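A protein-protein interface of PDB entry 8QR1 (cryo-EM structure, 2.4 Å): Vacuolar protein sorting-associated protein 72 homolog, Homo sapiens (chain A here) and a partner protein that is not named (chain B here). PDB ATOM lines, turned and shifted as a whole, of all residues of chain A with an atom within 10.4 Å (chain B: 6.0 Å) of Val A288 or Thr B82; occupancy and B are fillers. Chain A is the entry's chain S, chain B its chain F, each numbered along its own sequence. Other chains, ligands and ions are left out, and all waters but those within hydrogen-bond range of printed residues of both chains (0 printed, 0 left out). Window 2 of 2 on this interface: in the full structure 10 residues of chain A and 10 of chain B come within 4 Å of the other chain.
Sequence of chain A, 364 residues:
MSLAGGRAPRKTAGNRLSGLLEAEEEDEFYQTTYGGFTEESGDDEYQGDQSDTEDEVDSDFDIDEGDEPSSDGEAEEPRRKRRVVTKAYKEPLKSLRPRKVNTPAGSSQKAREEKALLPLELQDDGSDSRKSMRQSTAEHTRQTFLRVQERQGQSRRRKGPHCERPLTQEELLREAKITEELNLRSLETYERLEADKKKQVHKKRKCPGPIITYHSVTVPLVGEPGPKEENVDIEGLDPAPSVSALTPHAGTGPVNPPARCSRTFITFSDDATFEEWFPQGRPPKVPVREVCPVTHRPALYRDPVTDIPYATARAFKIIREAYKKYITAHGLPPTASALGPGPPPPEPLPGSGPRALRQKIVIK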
ATOM      1  N   PRO A 284      -4.853  34.410 -25.081  1.00  0.00           N
ATOM      2  CA  PRO A 284      -5.907  33.491 -25.521  1.00  0.00           C
ATOM      3  C   PRO A 284      -7.098  33.586 -24.589  1.00  0.00           C
ATOM      4  O   PRO A 284      -6.953  33.336 -23.388  1.00  0.00           O
ATOM      5  CB  PRO A 284      -5.233  32.117 -25.454  1.00  0.00           C
ATOM      6  CG  PRO A 284      -4.228  32.257 -24.378  1.00  0.00           C
ATOM      7  CD  PRO A 284      -3.764  33.692 -24.392  1.00  0.00           C
ATOM      8  N   LYS A 285      -8.269  33.942 -25.132  1.00  0.00           N
ATOM      9  CA  LYS A 285      -9.420  34.270 -24.294  1.00  0.00           C
ATOM     10  C   LYS A 285      -9.871  33.089 -23.451  1.00  0.00           C
ATOM     11  O   LYS A 285     -10.287  33.278 -22.301  1.00  0.00           O
ATOM     12  CB  LYS A 285     -10.584  34.758 -25.157  1.00  0.00           C
ATOM     13  CG  LYS A 285     -10.355  36.105 -25.824  1.00  0.00           C
ATOM     14  CD  LYS A 285     -11.366  36.375 -26.934  1.00  0.00           C
ATOM     15  CE  LYS A 285     -12.789  36.524 -26.397  1.00  0.00           C
ATOM     16  NZ  LYS A 285     -13.746  36.926 -27.461  1.00  0.00           N
ATOM     17  N   VAL A 286      -9.822  31.882 -24.015  1.00  0.00           N
ATOM     18  CA  VAL A 286     -10.147  30.645 -23.299  1.00  0.00           C
ATOM     19  C   VAL A 286      -9.114  29.583 -23.639  1.00  0.00           C
ATOM     20  O   VAL A 286      -8.427  29.666 -24.666  1.00  0.00           O
ATOM     21  CB  VAL A 286     -11.570  30.130 -23.648  1.00  0.00           C
ATOM     22  CG1 VAL A 286     -12.570  31.273 -23.665  1.00  0.00           C
ATOM     23  CG2 VAL A 286     -11.623  29.402 -25.013  1.00  0.00           C
ATOM     24  N   PRO A 287      -8.985  28.556 -22.789  1.00  0.00           N
ATOM     25  CA  PRO A 287      -8.079  27.448 -23.109  1.00  0.00           C
ATOM     26  C   PRO A 287      -8.802  26.362 -23.890  1.00  0.00           C
ATOM     27  O   PRO A 287     -10.008  26.424 -24.136  1.00  0.00           O
ATOM     28  CB  PRO A 287      -7.665  26.953 -21.728  1.00  0.00           C
ATOM     29  CG  PRO A 287      -8.934  27.089 -20.970  1.00  0.00           C
ATOM     30  CD  PRO A 287      -9.553  28.364 -21.438  1.00  0.00           C
ATOM     31  N   VAL A 288      -8.035  25.341 -24.274  1.00  0.00           N
ATOM     32  CA  VAL A 288      -8.645  24.113 -24.766  1.00  0.00           C
ATOM     33  C   VAL A 288      -9.269  23.377 -23.588  1.00  0.00           C
ATOM     34  O   VAL A 288      -8.629  23.166 -22.550  1.00  0.00           O
ATOM     35  CB  VAL A 288      -7.620  23.226 -25.499  1.00  0.00           C
ATOM     36  CG1 VAL A 288      -6.464  22.776 -24.583  1.00  0.00           C
ATOM     37  CG2 VAL A 288      -8.305  22.015 -26.129  1.00  0.00           C
ATOM     38  N   ARG A 289     -10.535  23.000 -23.736  1.00  0.00           N
ATOM     39  CA  ARG A 289     -11.236  22.233 -22.710  1.00  0.00           C
ATOM     40  C   ARG A 289     -10.784  20.784 -22.827  1.00  0.00           C
ATOM     41  O   ARG A 289     -11.042  20.120 -23.833  1.00  0.00           O
ATOM     42  CB  ARG A 289     -12.746  22.367 -22.874  1.00  0.00           C
ATOM     43  CG  ARG A 289     -13.285  23.744 -22.509  1.00  0.00           C
ATOM     44  CD  ARG A 289     -14.478  24.145 -23.370  1.00  0.00           C
ATOM     45  NE  ARG A 289     -15.626  23.265 -23.175  1.00  0.00           N
ATOM     46  CZ  ARG A 289     -16.782  23.356 -23.824  1.00  0.00           C
ATOM     47  NH1 ARG A 289     -17.000  24.282 -24.747  1.00  0.00           N
ATOM     48  NH2 ARG A 289     -17.752  22.491 -23.540  1.00  0.00           N
ATOM     49  N   GLU A 290     -10.122  20.288 -21.785  1.00  0.00           N
ATOM     50  CA  GLU A 290      -9.475  18.985 -21.854  1.00  0.00           C
ATOM     51  C   GLU A 290     -10.433  17.898 -21.390  1.00  0.00           C
ATOM     52  O   GLU A 290     -11.221  18.095 -20.461  1.00  0.00           O
ATOM     53  CB  GLU A 290      -8.182  18.917 -21.016  1.00  0.00           C
ATOM     54  CG  GLU A 290      -7.180  20.110 -20.999  1.00  0.00           C
ATOM     55  CD  GLU A 290      -7.672  21.376 -20.314  1.00  0.00           C
ATOM     56  OE1 GLU A 290      -6.902  22.358 -20.249  1.00  0.00           O
ATOM     57  OE2 GLU A 290      -8.829  21.385 -19.849  1.00  0.00           O
ATOM     58  N   VAL A 291     -10.358  16.747 -22.057  1.00  0.00           N
ATOM     59  CA  VAL A 291     -11.199  15.590 -21.783  1.00  0.00           C
ATOM     60  C   VAL A 291     -10.294  14.378 -21.630  1.00  0.00           C
ATOM     61  O   VAL A 291      -9.325  14.217 -22.380  1.00  0.00           O
ATOM     62  CB  VAL A 291     -12.231  15.358 -22.907  1.00  0.00           C
ATOM     63  CG1 VAL A 291     -13.029  14.082 -22.639  1.00  0.00           C
ATOM     64  CG2 VAL A 291     -13.147  16.575 -23.048  1.00  0.00           C
ATOM     65  N   CYS A 292     -10.603  13.536 -20.654  1.00  0.00           N
ATOM     66  CA  CYS A 292      -9.807  12.338 -20.433  1.00  0.00           C
ATOM     67  C   CYS A 292      -9.981  11.381 -21.613  1.00  0.00           C
ATOM     68  O   CYS A 292     -11.103  11.224 -22.106  1.00  0.00           O
ATOM     69  CB  CYS A 292     -10.229  11.654 -19.139  1.00  0.00           C
ATOM     70  SG  CYS A 292      -9.368  10.103 -18.819  1.00  0.00           S
ATOM     71  N   PRO A 298     -14.520  15.916 -17.779  1.00  0.00           N
ATOM     72  CA  PRO A 298     -13.419  16.887 -17.813  1.00  0.00           C
ATOM     73  C   PRO A 298     -12.174  16.368 -17.114  1.00  0.00           C
ATOM     74  O   PRO A 298     -12.244  15.571 -16.175  1.00  0.00           O
ATOM     75  CB  PRO A 298     -13.996  18.107 -17.087  1.00  0.00           C
ATOM     76  CG  PRO A 298     -15.454  17.962 -17.197  1.00  0.00           C
ATOM     77  CD  PRO A 298     -15.710  16.496 -17.129  1.00  0.00           C
ATOM     78  N   ALA A 299     -11.025  16.830 -17.596  1.00  0.00           N
ATOM     79  CA  ALA A 299      -9.753  16.414 -17.030  1.00  0.00           C
ATOM     80  C   ALA A 299      -9.611  16.909 -15.599  1.00  0.00           C
ATOM     81  O   ALA A 299     -10.172  17.938 -15.214  1.00  0.00           O
ATOM     82  CB  ALA A 299      -8.599  16.944 -17.874  1.00  0.00           C
ATOM     83  N   ARG A 302      -3.462  17.036 -13.505  1.00  0.00           N
ATOM     84  CA  ARG A 302      -2.818  17.561 -14.699  1.00  0.00           C
ATOM     85  C   ARG A 302      -2.456  16.342 -15.549  1.00  0.00           C
ATOM     86  O   ARG A 302      -2.995  15.248 -15.347  1.00  0.00           O
ATOM     87  CB  ARG A 302      -1.591  18.421 -14.331  1.00  0.00           C
ATOM     88  CG  ARG A 302      -1.836  19.859 -13.928  1.00  0.00           C
ATOM     89  CD  ARG A 302      -2.288  20.765 -15.066  1.00  0.00           C
ATOM     90  NE  ARG A 302      -3.602  21.314 -14.749  1.00  0.00           N
ATOM     91  CZ  ARG A 302      -3.824  22.229 -13.808  1.00  0.00           C
ATOM     92  NH1 ARG A 302      -2.834  22.895 -13.229  1.00  0.00           N
ATOM     93  NH2 ARG A 302      -5.070  22.476 -13.425  1.00  0.00           N
ATOM     94  N   ASP A 303      -1.545  16.519 -16.503  1.00  0.00           N
ATOM     95  CA  ASP A 303      -0.864  15.390 -17.119  1.00  0.00           C
ATOM     96  C   ASP A 303      -0.045  14.680 -16.044  1.00  0.00           C
ATOM     97  O   ASP A 303       0.270  15.285 -15.012  1.00  0.00           O
ATOM     98  CB  ASP A 303       0.059  15.832 -18.258  1.00  0.00           C
ATOM     99  CG  ASP A 303      -0.627  16.743 -19.254  1.00  0.00           C
ATOM    100  OD1 ASP A 303      -1.873  16.754 -19.283  1.00  0.00           O
ATOM    101  OD2 ASP A 303       0.081  17.445 -20.008  1.00  0.00           O
ATOM    102  N   PRO A 309      -3.525  14.301 -19.877  1.00  0.00           N
ATOM    103  CA  PRO A 309      -4.276  14.352 -18.619  1.00  0.00           C
ATOM    104  C   PRO A 309      -5.314  13.248 -18.502  1.00  0.00           C
ATOM    105  O   PRO A 309      -5.615  12.522 -19.452  1.00  0.00           O
ATOM    106  CB  PRO A 309      -4.938  15.731 -18.659  1.00  0.00           C
ATOM    107  CG  PRO A 309      -5.158  15.981 -20.073  1.00  0.00           C
ATOM    108  CD  PRO A 309      -4.050  15.301 -20.832  1.00  0.00           C
ATOM    109  N   PRO A 354      -4.027  10.281 -28.259  1.00  0.00           N
ATOM    110  CA  PRO A 354      -3.896  11.671 -28.721  1.00  0.00           C
ATOM    111  C   PRO A 354      -2.488  12.234 -28.625  1.00  0.00           C
ATOM    112  O   PRO A 354      -2.183  13.203 -29.332  1.00  0.00           O
ATOM    113  CB  PRO A 354      -4.845  12.433 -27.793  1.00  0.00           C
ATOM    114  CG  PRO A 354      -4.736  11.703 -26.524  1.00  0.00           C
ATOM    115  CD  PRO A 354      -4.597  10.246 -26.897  1.00  0.00           C
ATOM    116  N   GLN B  78     -17.172  29.622 -29.704  1.00  0.00           N
ATOM    117  CA  GLN B  78     -16.000  30.073 -28.963  1.00  0.00           C
ATOM    118  C   GLN B  78     -14.690  29.633 -29.613  1.00  0.00           C
ATOM    119  O   GLN B  78     -13.662  29.577 -28.930  1.00  0.00           O
ATOM    120  CB  GLN B  78     -16.052  29.556 -27.518  1.00  0.00           C
ATOM    121  CG  GLN B  78     -17.312  29.848 -26.653  1.00  0.00           C
ATOM    122  CD  GLN B  78     -18.205  30.985 -27.136  1.00  0.00           C
ATOM    123  OE1 GLN B  78     -19.405  30.798 -27.335  1.00  0.00           O
ATOM    124  NE2 GLN B  78     -17.638  32.178 -27.255  1.00  0.00           N
ATOM    125  N   GLY B  79     -14.703  29.325 -30.906  1.00  0.00           N
ATOM    126  CA  GLY B  79     -13.521  28.886 -31.615  1.00  0.00           C
ATOM    127  C   GLY B  79     -13.365  27.376 -31.619  1.00  0.00           C
ATOM    128  O   GLY B  79     -13.887  26.656 -30.770  1.00  0.00           O
ATOM    129  N   TYR B  80     -12.619  26.893 -32.616  1.00  0.00           N
ATOM    130  CA  TYR B  80     -12.396  25.458 -32.748  1.00  0.00           C
ATOM    131  C   TYR B  80     -11.394  24.948 -31.720  1.00  0.00           C
ATOM    132  O   TYR B  80     -11.542  23.834 -31.204  1.00  0.00           O
ATOM    133  CB  TYR B  80     -11.913  25.127 -34.157  1.00  0.00           C
ATOM    134  CG  TYR B  80     -11.280  23.761 -34.268  1.00  0.00           C
ATOM    135  CD1 TYR B  80     -12.032  22.611 -34.097  1.00  0.00           C
ATOM    136  CD2 TYR B  80      -9.927  23.621 -34.524  1.00  0.00           C
ATOM    137  CE1 TYR B  80     -11.456  21.363 -34.191  1.00  0.00           C
ATOM    138  CE2 TYR B  80      -9.344  22.377 -34.618  1.00  0.00           C
ATOM    139  CZ  TYR B  80     -10.112  21.252 -34.451  1.00  0.00           C
ATOM    140  OH  TYR B  80      -9.530  20.011 -34.542  1.00  0.00           O
ATOM    141  N   ARG B  81     -10.368  25.744 -31.410  1.00  0.00           N
ATOM    142  CA  ARG B  81      -9.341  25.287 -30.474  1.00  0.00           C
ATOM    143  C   ARG B  81      -9.898  25.126 -29.066  1.00  0.00           C
ATOM    144  O   ARG B  81      -9.336  24.377 -28.259  1.00  0.00           O
ATOM    145  CB  ARG B  81      -8.149  26.251 -30.454  1.00  0.00           C
ATOM    146  CG  ARG B  81      -6.861  25.682 -31.055  1.00  0.00           C
ATOM    147  CD  ARG B  81      -6.915  25.618 -32.584  1.00  0.00           C
ATOM    148  NE  ARG B  81      -5.949  24.674 -33.140  1.00  0.00           N
ATOM    149  CZ  ARG B  81      -5.621  24.577 -34.424  1.00  0.00           C
ATOM    150  NH1 ARG B  81      -6.150  25.370 -35.347  1.00  0.00           N
ATOM    151  NH2 ARG B  81      -4.736  23.658 -34.797  1.00  0.00           N
ATOM    152  N   THR B  82     -10.992  25.822 -28.749  1.00  0.00           N
ATOM    153  CA  THR B  82     -11.659  25.627 -27.468  1.00  0.00           C
ATOM    154  C   THR B  82     -12.181  24.202 -27.327  1.00  0.00           C
ATOM    155  O   THR B  82     -12.125  23.622 -26.236  1.00  0.00           O
ATOM    156  CB  THR B  82     -12.805  26.627 -27.331  1.00  0.00           C
ATOM    157  OG1 THR B  82     -12.310  27.955 -27.537  1.00  0.00           O
ATOM    158  CG2 THR B  82     -13.446  26.533 -25.961  1.00  0.00           C
ATOM    159  N   VAL B  83     -12.681  23.622 -28.423  1.00  0.00           N
ATOM    160  CA  VAL B  83     -13.381  22.344 -28.432  1.00  0.00           C
ATOM    161  C   VAL B  83     -12.699  21.320 -29.331  1.00  0.00           C
ATOM    162  O   VAL B  83     -13.362  20.421 -29.844  1.00  0.00           O
ATOM    163  CB  VAL B  83     -14.856  22.522 -28.844  1.00  0.00           C
ATOM    164  CG1 VAL B  83     -15.562  23.475 -27.903  1.00  0.00           C
ATOM    165  CG2 VAL B  83     -14.992  22.998 -30.292  1.00  0.00           C
ATOM    166  N   LYS B  84     -11.385  21.434 -29.536  1.00  0.00           N
ATOM    167  CA  LYS B  84     -10.715  20.506 -30.443  1.00  0.00           C
ATOM    168  C   LYS B  84     -10.659  19.101 -29.855  1.00  0.00           C
ATOM    169  O   LYS B  84     -10.820  18.114 -30.579  1.00  0.00           O
ATOM    170  CB  LYS B  84      -9.317  21.029 -30.804  1.00  0.00           C
ATOM    171  CG  LYS B  84      -8.243  21.047 -29.705  1.00  0.00           C
ATOM    172  CD  LYS B  84      -6.855  21.271 -30.305  1.00  0.00           C
ATOM    173  CE  LYS B  84      -5.743  21.070 -29.284  1.00  0.00           C
ATOM    174  NZ  LYS B  84      -4.406  20.949 -29.933  1.00  0.00           N
ATOM    175  N   ALA B  85     -10.451  18.991 -28.543  1.00  0.00           N
ATOM    176  CA  ALA B  85     -10.355  17.677 -27.918  1.00  0.00           C
ATOM    177  C   ALA B  85     -11.710  16.990 -27.841  1.00  0.00           C
ATOM    178  O   ALA B  85     -11.800  15.772 -28.044  1.00  0.00           O
ATOM    179  CB  ALA B  85      -9.752  17.808 -26.522  1.00  0.00           C
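The backbone NH of Arg A289 sits at hydrogen-bond distance from the backbone carbonyl oxygen of Thr B82 (3.0 Å).
The side-chain hydroxyl (OG1) of Thr B82 sits at hydrogen-bond distance from the backbone carbonyl oxygen (O) of Gln B78, 2.5 Å away.
Among the printed residues, merely in contact across the chains: Val A286 with Thr B82 (3.0 Å), Val A288 with Arg B81 (3.3 Å), Arg A289 with Val B83 (3.6 Å), Val A288 with Lys B84 (3.7 Å), Arg A289 with Ala B85 (3.8 Å), Pro A287 with Thr B82 (3.8 Å) and Val A288 with Thr B82 (3.8 Å).
Thr B82 touches just these residues of chain A: Val A286, Pro A287, Val A288 and Arg A289. Val B83 touches one residue of chain A. Printed residues of chain A within 4 Å of Arg B81: Val A288 (3.3 Å). Of the printed residues of chain A, Ala B85 touches Arg A289. Of the printed residues of chain B, Arg A289 touches Thr B82, Val B83 and Ala B85. Of the printed residues of chain B, Val A286 touches Thr B82. Printed residues of chain B within 4 Å of Pro A287: Thr B82 (3.8 Å). Lys A285 touches none of the printed residues of chain B. Pro A298 touches none of the printed residues of chain B.
Of the 15 printed residues of chain A, 4 touch a printed residue of chain B. Along chain A the printed residues that touch a printed residue of chain B span positions 286 to 289. Among the printed residues, 8 pairs touch across the chains. Among the printed residues, no Asp or Glu carboxylate lies within 4 Å of a Lys or Arg side-chain nitrogen of the other chain.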
